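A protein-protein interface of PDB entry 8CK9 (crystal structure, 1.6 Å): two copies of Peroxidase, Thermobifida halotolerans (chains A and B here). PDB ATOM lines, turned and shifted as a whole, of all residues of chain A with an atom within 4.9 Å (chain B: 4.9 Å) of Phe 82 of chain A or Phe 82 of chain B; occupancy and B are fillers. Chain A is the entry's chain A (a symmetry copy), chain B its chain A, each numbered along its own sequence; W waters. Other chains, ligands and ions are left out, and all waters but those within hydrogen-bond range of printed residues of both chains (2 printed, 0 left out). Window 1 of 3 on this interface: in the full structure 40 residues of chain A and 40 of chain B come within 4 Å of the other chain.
The side-chain carboxylate (OD1) of Asp 190 of chain B lies within hydrogen-bond range of the side-chain hydroxyl (OG1) of Thr 221 of chain A (2.7 Å).
OD1 of Asp 190 of chain A lies within hydrogen-bond range of OG1 of Thr 221 of chain B, 2.7 Å away.
The backbone NH (N) of Phe 82 of chain B is in hydrogen-bond range of the backbone carbonyl oxygen (O) of Ala 188 of chain B.
The backbone carbonyl oxygen (O) of Ala 188 of chain A lies within hydrogen-bond range of the backbone NH (N) of Phe 82 of chain A, at 2.9 Å.
Phe 82 of chain A touches Phe 82 of chain B.
Pro 191 of chain B touches Phe 82 of chain A (CG to CE1, 3.8 Å).
Pro 191 of chain A touches Phe 82 of chain B (CG to CE1, 3.8 Å).
Pro 191 of chain A touches Phe 218 of chain B (CB to CD2, 3.8 Å).
Pro 191 of chain A touches Thr 221 of chain B.
Pro 191 of chain B touches Phe 218 of chain A (CB to CD2, 3.8 Å).
Thr 221 of chain A touches Pro 191 of chain B.
Of chain B, only Phe 82 (3.3 Å) and Pro 191 (3.8 Å) come within 4 Å of Phe 82 of chain A.
Of the printed residues of chain A, Phe 82 of chain B touches Phe 82 and Pro 191.
Of the printed residues of chain A, Asp 190 of chain B touches Thr 221 (2.7 Å).
Printed residues of chain A within 4 Å of Phe 218 of chain B: Pro 191.
Leu 194 of chain B touches none of the printed residues of chain A.
Of the 16 printed residues of chain A, 5 touch a printed residue of chain B.
Printed residues of chain A that touch a printed residue of chain B: Phe 82, Asp 190, Pro 191, Phe 218 and Thr 221.
Hydrophobic or aromatic side chains of chain B that line the printed part of chain A: Phe 82, Pro 191 and Phe 218.
Among the printed residues, no Asp or Glu carboxylate lies within 4 Å of a Lys or Arg side-chain nitrogen of the other chain.
Phe 82 of chain B touches its own counterpart, Phe 82 of chain A.
Phe 82 of chain A touches Pro 191 of chain B, and with the chains exchanged Pro 191 of chain A touches Phe 82 of chain B.
Asp 190 of chain A touches Thr 221 of chain B, and with the chains exchanged Thr 221 of chain A touches Asp 190 of chain B.
Pro 191 of chain A touches Thr 221 of chain B, and with the chains exchanged Thr 221 of chain A touches Pro 191 of chain B.
Positions printed for both chains: 80, 81, 82, 83, 84, 186, 187, 188, 189, 190, 191, 194, 217, 218, 221 and 355.
Of the 9 pairs that touch across the chains among the printed residues, 9 have their exchanged pair printed and touching as well.
Water W1 bridges O of Glu 189 of chain B (2.8 Å) and OG1 of Thr 221 of chain A (2.9 Å).
Water W2 lies within hydrogen-bond range of the backbone carbonyl oxygen of Glu 189 of chain A (2.8 Å) and the side-chain hydroxyl of Thr 221 of chain B (2.9 Å).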
ATOM      1  N   PRO A  80      11.210 -15.031   6.599  1.00  0.00           N
ATOM      2  CA  PRO A  80      10.769 -13.675   6.919  1.00  0.00           C
ATOM      3  C   PRO A  80      11.903 -12.673   6.794  1.00  0.00           C
ATOM      4  O   PRO A  80      13.080 -13.023   6.812  1.00  0.00           O
ATOM      5  CB  PRO A  80      10.300 -13.793   8.376  1.00  0.00           C
ATOM      6  CG  PRO A  80      10.023 -15.254   8.580  1.00  0.00           C
ATOM      7  CD  PRO A  80      11.056 -15.946   7.743  1.00  0.00           C
ATOM      8  N   ALA A  81      11.512 -11.396   6.703  1.00  0.00           N
ATOM      9  CA  ALA A  81      12.471 -10.315   6.497  1.00  0.00           C
ATOM     10  C   ALA A  81      13.396 -10.082   7.691  1.00  0.00           C
ATOM     11  O   ALA A  81      14.504  -9.573   7.508  1.00  0.00           O
ATOM     12  CB  ALA A  81      11.725  -9.020   6.165  1.00  0.00           C
ATOM     13  N   PHE A  82      12.982 -10.428   8.914  1.00  0.00           N
ATOM     14  CA  PHE A  82      13.783 -10.149  10.099  1.00  0.00           C
ATOM     15  C   PHE A  82      14.044 -11.417  10.895  1.00  0.00           C
ATOM     16  O   PHE A  82      13.231 -12.345  10.906  1.00  0.00           O
ATOM     17  CB  PHE A  82      13.101  -9.101  10.999  1.00  0.00           C
ATOM     18  CG  PHE A  82      12.813  -7.828  10.283  1.00  0.00           C
ATOM     19  CD1 PHE A  82      13.799  -6.870  10.141  1.00  0.00           C
ATOM     20  CD2 PHE A  82      11.579  -7.630   9.688  1.00  0.00           C
ATOM     21  CE1 PHE A  82      13.544  -5.695   9.438  1.00  0.00           C
ATOM     22  CE2 PHE A  82      11.314  -6.463   8.982  1.00  0.00           C
ATOM     23  CZ  PHE A  82      12.297  -5.504   8.860  1.00  0.00           C
ATOM     24  N   VAL A  83      15.189 -11.440  11.577  1.00  0.00           N
ATOM     25  CA  VAL A  83      15.548 -12.544  12.461  1.00  0.00           C
ATOM     26  C   VAL A  83      16.188 -11.975  13.719  1.00  0.00           C
ATOM     27  O   VAL A  83      16.816 -10.911  13.710  1.00  0.00           O
ATOM     28  CB  VAL A  83      16.497 -13.568  11.776  1.00  0.00           C
ATOM     29  CG1 VAL A  83      17.950 -13.038  11.697  1.00  0.00           C
ATOM     30  CG2 VAL A  83      16.440 -14.939  12.488  1.00  0.00           C
ATOM     31  N   HIS A  84      16.012 -12.695  14.821  1.00  0.00           N
ATOM     32  CA  HIS A  84      16.763 -12.446  16.036  1.00  0.00           C
ATOM     33  C   HIS A  84      17.306 -13.794  16.464  1.00  0.00           C
ATOM     34  O   HIS A  84      16.529 -14.717  16.728  1.00  0.00           O
ATOM     35  CB  HIS A  84      15.885 -11.818  17.125  1.00  0.00           C
ATOM     36  CG  HIS A  84      16.657 -11.078  18.166  1.00  0.00           C
ATOM     37  ND1 HIS A  84      16.074 -10.137  18.988  1.00  0.00           N
ATOM     38  CD2 HIS A  84      17.962 -11.136  18.521  1.00  0.00           C
ATOM     39  CE1 HIS A  84      16.988  -9.651  19.812  1.00  0.00           C
ATOM     40  NE2 HIS A  84      18.141 -10.241  19.553  1.00  0.00           N
ATOM     41  N   ILE A 186      14.297 -16.528  16.186  1.00  0.00           N
ATOM     42  CA  ILE A 186      12.974 -15.925  16.109  1.00  0.00           C
ATOM     43  C   ILE A 186      12.905 -15.139  14.814  1.00  0.00           C
ATOM     44  O   ILE A 186      13.794 -14.328  14.534  1.00  0.00           O
ATOM     45  CB  ILE A 186      12.690 -15.012  17.314  1.00  0.00           C
ATOM     46  CG1 ILE A 186      13.103 -15.690  18.629  1.00  0.00           C
ATOM     47  CG2 ILE A 186      11.225 -14.615  17.333  1.00  0.00           C
ATOM     48  CD1 ILE A 186      13.032 -14.764  19.821  1.00  0.00           C
ATOM     49  N   GLY A 187      11.876 -15.385  14.018  1.00  0.00           N
ATOM     50  CA  GLY A 187      11.727 -14.701  12.748  1.00  0.00           C
ATOM     51  C   GLY A 187      10.358 -14.069  12.629  1.00  0.00           C
ATOM     52  O   GLY A 187       9.370 -14.573  13.168  1.00  0.00           O
ATOM     53  N   ALA A 188      10.312 -12.941  11.921  1.00  0.00           N
ATOM     54  CA  ALA A 188       9.040 -12.309  11.597  1.00  0.00           C
ATOM     55  C   ALA A 188       9.253 -11.319  10.465  1.00  0.00           C
ATOM     56  O   ALA A 188      10.383 -10.899  10.182  1.00  0.00           O
ATOM     57  CB  ALA A 188       8.433 -11.601  12.818  1.00  0.00           C
ATOM     58  N   GLU A 189       8.152 -10.959   9.810  1.00  0.00           N
ATOM     59  CA  GLU A 189       8.188  -9.996   8.709  1.00  0.00           C
ATOM     60  C   GLU A 189       8.109  -8.556   9.203  1.00  0.00           C
ATOM     61  O   GLU A 189       8.226  -7.615   8.402  1.00  0.00           O
ATOM     62  CB  GLU A 189       7.048 -10.300   7.733  1.00  0.00           C
ATOM     63  CG  GLU A 189       7.077  -9.510   6.420  1.00  0.00           C
ATOM     64  CD  GLU A 189       8.234  -9.866   5.496  1.00  0.00           C
ATOM     65  OE1 GLU A 189       8.881 -10.919   5.665  1.00  0.00           O
ATOM     66  OE2 GLU A 189       8.491  -9.054   4.573  1.00  0.00           O
ATOM     67  N   ASP A 190       7.940  -8.366  10.505  1.00  0.00           N
ATOM     68  CA  ASP A 190       7.819  -7.059  11.109  1.00  0.00           C
ATOM     69  C   ASP A 190       8.698  -6.957  12.349  1.00  0.00           C
ATOM     70  O   ASP A 190       8.712  -7.876  13.181  1.00  0.00           O
ATOM     71  CB  ASP A 190       6.365  -6.793  11.490  1.00  0.00           C
ATOM     72  CG  ASP A 190       6.183  -5.423  12.051  1.00  0.00           C
ATOM     73  OD1 ASP A 190       5.927  -4.498  11.252  1.00  0.00           O
ATOM     74  OD2 ASP A 190       6.339  -5.271  13.277  1.00  0.00           O
ATOM     75  N   PRO A 191       9.429  -5.848  12.509  1.00  0.00           N
ATOM     76  CA  PRO A 191      10.377  -5.744  13.629  1.00  0.00           C
ATOM     77  C   PRO A 191       9.710  -5.572  14.975  1.00  0.00           C
ATOM     78  O   PRO A 191      10.312  -5.925  15.995  1.00  0.00           O
ATOM     79  CB  PRO A 191      11.209  -4.511  13.256  1.00  0.00           C
ATOM     80  CG  PRO A 191      10.237  -3.663  12.484  1.00  0.00           C
ATOM     81  CD  PRO A 191       9.473  -4.649  11.650  1.00  0.00           C
ATOM     82  N   LEU A 194       8.567  -9.042  16.001  1.00  0.00           N
ATOM     83  CA  LEU A 194       9.770  -9.743  16.438  1.00  0.00           C
ATOM     84  C   LEU A 194      10.194  -9.292  17.828  1.00  0.00           C
ATOM     85  O   LEU A 194      10.484 -10.120  18.702  1.00  0.00           O
ATOM     86  CB  LEU A 194      10.886  -9.498  15.422  1.00  0.00           C
ATOM     87  CG  LEU A 194      12.202 -10.183  15.781  1.00  0.00           C
ATOM     88  CD1 LEU A 194      12.014 -11.671  15.685  1.00  0.00           C
ATOM     89  CD2 LEU A 194      13.337  -9.713  14.876  1.00  0.00           C
ATOM     90  N   GLY A 217      19.138  -9.638  12.582  1.00  0.00           N
ATOM     91  CA  GLY A 217      19.459  -9.624  11.173  1.00  0.00           C
ATOM     92  C   GLY A 217      18.258  -9.229  10.336  1.00  0.00           C
ATOM     93  O   GLY A 217      17.116  -9.261  10.798  1.00  0.00           O
ATOM     94  N   PHE A 218      18.532  -8.863   9.080  1.00  0.00           N
ATOM     95  CA  PHE A 218      17.463  -8.420   8.200  1.00  0.00           C
ATOM     96  C   PHE A 218      17.761  -8.783   6.752  1.00  0.00           C
ATOM     97  O   PHE A 218      18.915  -8.984   6.354  1.00  0.00           O
ATOM     98  CB  PHE A 218      17.227  -6.900   8.312  1.00  0.00           C
ATOM     99  CG  PHE A 218      18.449  -6.072   8.006  1.00  0.00           C
ATOM    100  CD1 PHE A 218      19.400  -5.825   8.977  1.00  0.00           C
ATOM    101  CD2 PHE A 218      18.638  -5.544   6.740  1.00  0.00           C
ATOM    102  CE1 PHE A 218      20.533  -5.056   8.694  1.00  0.00           C
ATOM    103  CE2 PHE A 218      19.768  -4.775   6.453  1.00  0.00           C
ATOM    104  CZ  PHE A 218      20.709  -4.541   7.427  1.00  0.00           C
ATOM    105  N   THR A 221      12.217  -6.391   2.819  1.00  0.00           N
ATOM    106  CA  THR A 221      10.847  -6.771   3.119  1.00  0.00           C
ATOM    107  C   THR A 221      10.113  -7.128   1.835  1.00  0.00           C
ATOM    108  O   THR A 221      10.371  -6.568   0.767  1.00  0.00           O
ATOM    109  CB  THR A 221      10.086  -5.651   3.838  1.00  0.00           C
ATOM    110  OG1 THR A 221      10.015  -4.497   2.986  1.00  0.00           O
ATOM    111  CG2 THR A 221      10.753  -5.282   5.166  1.00  0.00           C
ATOM    112  N   TYR A 355      21.044 -13.850   6.887  1.00  0.00           N
ATOM    113  CA  TYR A 355      20.530 -12.500   7.060  1.00  0.00           C
ATOM    114  C   TYR A 355      21.700 -11.534   7.091  1.00  0.00           C
ATOM    115  O   TYR A 355      22.827 -11.908   7.405  1.00  0.00           O
ATOM    116  CB  TYR A 355      19.696 -12.369   8.353  1.00  0.00           C
ATOM    117  CG  TYR A 355      18.364 -13.053   8.222  1.00  0.00           C
ATOM    118  CD1 TYR A 355      18.251 -14.437   8.347  1.00  0.00           C
ATOM    119  CD2 TYR A 355      17.221 -12.320   7.936  1.00  0.00           C
ATOM    120  CE1 TYR A 355      17.030 -15.074   8.182  1.00  0.00           C
ATOM    121  CE2 TYR A 355      15.998 -12.942   7.764  1.00  0.00           C
ATOM    122  CZ  TYR A 355      15.911 -14.315   7.886  1.00  0.00           C
ATOM    123  OH  TYR A 355      14.700 -14.950   7.714  1.00  0.00           O
ATOM    124  N   PRO B  80       8.397   6.928   7.930  1.00  0.00           N
ATOM    125  CA  PRO B  80       8.729   5.562   7.528  1.00  0.00           C
ATOM    126  C   PRO B  80       9.007   4.675   8.729  1.00  0.00           C
ATOM    127  O   PRO B  80       9.295   5.145   9.827  1.00  0.00           O
ATOM    128  CB  PRO B  80       9.994   5.744   6.677  1.00  0.00           C
ATOM    129  CG  PRO B  80       9.967   7.181   6.242  1.00  0.00           C
ATOM    130  CD  PRO B  80       9.361   7.908   7.404  1.00  0.00           C
ATOM    131  N   ALA B  81       8.950   3.362   8.478  1.00  0.00           N
ATOM    132  CA  ALA B  81       9.114   2.372   9.539  1.00  0.00           C
ATOM    133  C   ALA B  81      10.524   2.332  10.125  1.00  0.00           C
ATOM    134  O   ALA B  81      10.688   1.926  11.279  1.00  0.00           O
ATOM    135  CB  ALA B  81       8.734   0.986   9.014  1.00  0.00           C
ATOM    136  N   PHE B  82      11.555   2.729   9.373  1.00  0.00           N
ATOM    137  CA  PHE B  82      12.930   2.628   9.846  1.00  0.00           C
ATOM    138  C   PHE B  82      13.631   3.975   9.783  1.00  0.00           C
ATOM    139  O   PHE B  82      13.335   4.810   8.927  1.00  0.00           O
ATOM    140  CB  PHE B  82      13.724   1.589   9.032  1.00  0.00           C
ATOM    141  CG  PHE B  82      13.094   0.241   9.047  1.00  0.00           C
ATOM    142  CD1 PHE B  82      13.313  -0.620  10.108  1.00  0.00           C
ATOM    143  CD2 PHE B  82      12.223  -0.130   8.038  1.00  0.00           C
ATOM    144  CE1 PHE B  82      12.693  -1.866  10.144  1.00  0.00           C
ATOM    145  CE2 PHE B  82      11.596  -1.371   8.065  1.00  0.00           C
ATOM    146  CZ  PHE B  82      11.833  -2.230   9.117  1.00  0.00           C
ATOM    147  N   VAL B  83      14.581   4.169  10.698  1.00  0.00           N
ATOM    148  CA  VAL B  83      15.409   5.369  10.719  1.00  0.00           C
ATOM    149  C   VAL B  83      16.842   4.970  11.041  1.00  0.00           C
ATOM    150  O   VAL B  83      17.105   3.979  11.729  1.00  0.00           O
ATOM    151  CB  VAL B  83      14.892   6.430  11.733  1.00  0.00           C
ATOM    152  CG1 VAL B  83      15.248   6.046  13.192  1.00  0.00           C
ATOM    153  CG2 VAL B  83      15.419   7.838  11.380  1.00  0.00           C
ATOM    154  N   HIS B  84      17.779   5.752  10.519  1.00  0.00           N
ATOM    155  CA  HIS B  84      19.167   5.678  10.934  1.00  0.00           C
ATOM    156  C   HIS B  84      19.580   7.105  11.235  1.00  0.00           C
ATOM    157  O   HIS B  84      19.536   7.961  10.346  1.00  0.00           O
ATOM    158  CB  HIS B  84      20.050   5.052   9.849  1.00  0.00           C
ATOM    159  CG  HIS B  84      21.326   4.478  10.369  1.00  0.00           C
ATOM    160  ND1 HIS B  84      22.061   3.549   9.663  1.00  0.00           N
ATOM    161  CD2 HIS B  84      22.000   4.699  11.522  1.00  0.00           C
ATOM    162  CE1 HIS B  84      23.140   3.228  10.357  1.00  0.00           C
ATOM    163  NE2 HIS B  84      23.129   3.911  11.487  1.00  0.00           N
ATOM    164  N   ILE B 186      18.249   9.483   8.205  1.00  0.00           N
ATOM    165  CA  ILE B 186      17.893   8.743   7.003  1.00  0.00           C
ATOM    166  C   ILE B 186      16.714   7.855   7.346  1.00  0.00           C
ATOM    167  O   ILE B 186      16.760   7.121   8.339  1.00  0.00           O
ATOM    168  CB  ILE B 186      19.072   7.904   6.479  1.00  0.00           C
ATOM    169  CG1 ILE B 186      20.372   8.721   6.470  1.00  0.00           C
ATOM    170  CG2 ILE B 186      18.749   7.359   5.099  1.00  0.00           C
ATOM    171  CD1 ILE B 186      21.592   7.891   6.154  1.00  0.00           C
ATOM    172  N   GLY B 187      15.656   7.931   6.552  1.00  0.00           N
ATOM    173  CA  GLY B 187      14.470   7.137   6.804  1.00  0.00           C
ATOM    174  C   GLY B 187      14.064   6.360   5.571  1.00  0.00           C
ATOM    175  O   GLY B 187      14.273   6.799   4.438  1.00  0.00           O
ATOM    176  N   ALA B 188      13.489   5.181   5.806  1.00  0.00           N
ATOM    177  CA  ALA B 188      12.913   4.396   4.720  1.00  0.00           C
ATOM    178  C   ALA B 188      11.983   3.348   5.307  1.00  0.00           C
ATOM    179  O   ALA B 188      12.049   3.027   6.500  1.00  0.00           O
ATOM    180  CB  ALA B 188      14.000   3.728   3.866  1.00  0.00           C
ATOM    181  N   GLU B 189      11.105   2.826   4.454  1.00  0.00           N
ATOM    182  CA  GLU B 189      10.157   1.789   4.859  1.00  0.00           C
ATOM    183  C   GLU B 189      10.759   0.392   4.764  1.00  0.00           C
ATOM    184  O   GLU B 189      10.117  -0.592   5.165  1.00  0.00           O
ATOM    185  CB  GLU B 189       8.893   1.896   4.002  1.00  0.00           C
ATOM    186  CG  GLU B 189       7.721   1.013   4.444  1.00  0.00           C
ATOM    187  CD  GLU B 189       7.097   1.412   5.776  1.00  0.00           C
ATOM    188  OE1 GLU B 189       7.319   2.536   6.268  1.00  0.00           O
ATOM    189  OE2 GLU B 189       6.362   0.561   6.333  1.00  0.00           O
ATOM    190  N   ASP B 190      11.985   0.288   4.268  1.00  0.00           N
ATOM    191  CA  ASP B 190      12.669  -0.972   4.092  1.00  0.00           C
ATOM    192  C   ASP B 190      14.098  -0.887   4.611  1.00  0.00           C
ATOM    193  O   ASP B 190      14.806   0.092   4.329  1.00  0.00           O
ATOM    194  CB  ASP B 190      12.684  -1.357   2.615  1.00  0.00           C
ATOM    195  CG  ASP B 190      13.317  -2.690   2.397  1.00  0.00           C
ATOM    196  OD1 ASP B 190      12.578  -3.697   2.438  1.00  0.00           O
ATOM    197  OD2 ASP B 190      14.550  -2.727   2.230  1.00  0.00           O
ATOM    198  N   PRO B 191      14.556  -1.898   5.358  1.00  0.00           N
ATOM    199  CA  PRO B 191      15.889  -1.814   5.975  1.00  0.00           C
ATOM    200  C   PRO B 191      17.025  -1.948   4.987  1.00  0.00           C
ATOM    201  O   PRO B 191      18.124  -1.457   5.265  1.00  0.00           O
ATOM    202  CB  PRO B 191      15.874  -2.981   6.971  1.00  0.00           C
ATOM    203  CG  PRO B 191      14.968  -3.983   6.312  1.00  0.00           C
ATOM    204  CD  PRO B 191      13.866  -3.149   5.725  1.00  0.00           C
ATOM    205  N   LEU B 194      17.355   1.454   3.342  1.00  0.00           N
ATOM    206  CA  LEU B 194      18.015   2.308   4.324  1.00  0.00           C
ATOM    207  C   LEU B 194      19.507   2.014   4.394  1.00  0.00           C
ATOM    208  O   LEU B 194      20.335   2.934   4.373  1.00  0.00           O
ATOM    209  CB  LEU B 194      17.354   2.100   5.688  1.00  0.00           C
ATOM    210  CG  LEU B 194      17.970   2.944   6.801  1.00  0.00           C
ATOM    211  CD1 LEU B 194      17.677   4.393   6.530  1.00  0.00           C
ATOM    212  CD2 LEU B 194      17.445   2.524   8.171  1.00  0.00           C
ATOM    213  N   GLY B 217      16.758   2.867  14.362  1.00  0.00           N
ATOM    214  CA  GLY B 217      15.489   2.776  15.049  1.00  0.00           C
ATOM    215  C   GLY B 217      14.415   2.194  14.152  1.00  0.00           C
ATOM    216  O   GLY B 217      14.558   2.145  12.928  1.00  0.00           O
ATOM    217  N   PHE B 218      13.318   1.762  14.780  1.00  0.00           N
ATOM    218  CA  PHE B 218      12.240   1.142  14.025  1.00  0.00           C
ATOM    219  C   PHE B 218      10.890   1.419  14.671  1.00  0.00           C
ATOM    220  O   PHE B 218      10.787   1.706  15.869  1.00  0.00           O
ATOM    221  CB  PHE B 218      12.443  -0.380  13.887  1.00  0.00           C
ATOM    222  CG  PHE B 218      12.553  -1.099  15.208  1.00  0.00           C
ATOM    223  CD1 PHE B 218      13.758  -1.170  15.880  1.00  0.00           C
ATOM    224  CD2 PHE B 218      11.441  -1.703  15.770  1.00  0.00           C
ATOM    225  CE1 PHE B 218      13.859  -1.837  17.104  1.00  0.00           C
ATOM    226  CE2 PHE B 218      11.538  -2.372  16.994  1.00  0.00           C
ATOM    227  CZ  PHE B 218      12.742  -2.430  17.654  1.00  0.00           C
ATOM    228  N   THR B 221       5.920  -1.833  10.590  1.00  0.00           N
ATOM    229  CA  THR B 221       5.814  -1.574   9.164  1.00  0.00           C
ATOM    230  C   THR B 221       4.353  -1.396   8.777  1.00  0.00           C
ATOM    231  O   THR B 221       3.453  -2.011   9.355  1.00  0.00           O
ATOM    232  CB  THR B 221       6.422  -2.708   8.330  1.00  0.00           C
ATOM    233  OG1 THR B 221       5.705  -3.925   8.580  1.00  0.00           O
ATOM    234  CG2 THR B 221       7.908  -2.899   8.643  1.00  0.00           C
ATOM    235  N   TYR B 355      11.350   6.794  17.388  1.00  0.00           N
ATOM    236  CA  TYR B 355      11.521   5.416  16.954  1.00  0.00           C
ATOM    237  C   TYR B 355      11.956   4.581  18.145  1.00  0.00           C
ATOM    238  O   TYR B 355      12.511   5.093  19.114  1.00  0.00           O
ATOM    239  CB  TYR B 355      12.560   5.300  15.817  1.00  0.00           C
ATOM    240  CG  TYR B 355      12.018   5.831  14.519  1.00  0.00           C
ATOM    241  CD1 TYR B 355      11.965   7.202  14.269  1.00  0.00           C
ATOM    242  CD2 TYR B 355      11.522   4.965  13.557  1.00  0.00           C
ATOM    243  CE1 TYR B 355      11.424   7.694  13.091  1.00  0.00           C
ATOM    244  CE2 TYR B 355      10.975   5.442  12.380  1.00  0.00           C
ATOM    245  CZ  TYR B 355      10.927   6.804  12.155  1.00  0.00           C
ATOM    246  OH  TYR B 355      10.383   7.294  10.989  1.00  0.00           O
HETATM  247  O   HOH W   1       8.326  -2.545   4.234  1.00  0.00           O
HETATM  248  O   HOH W   2       6.665  -5.937   6.777  1.00  0.00           O
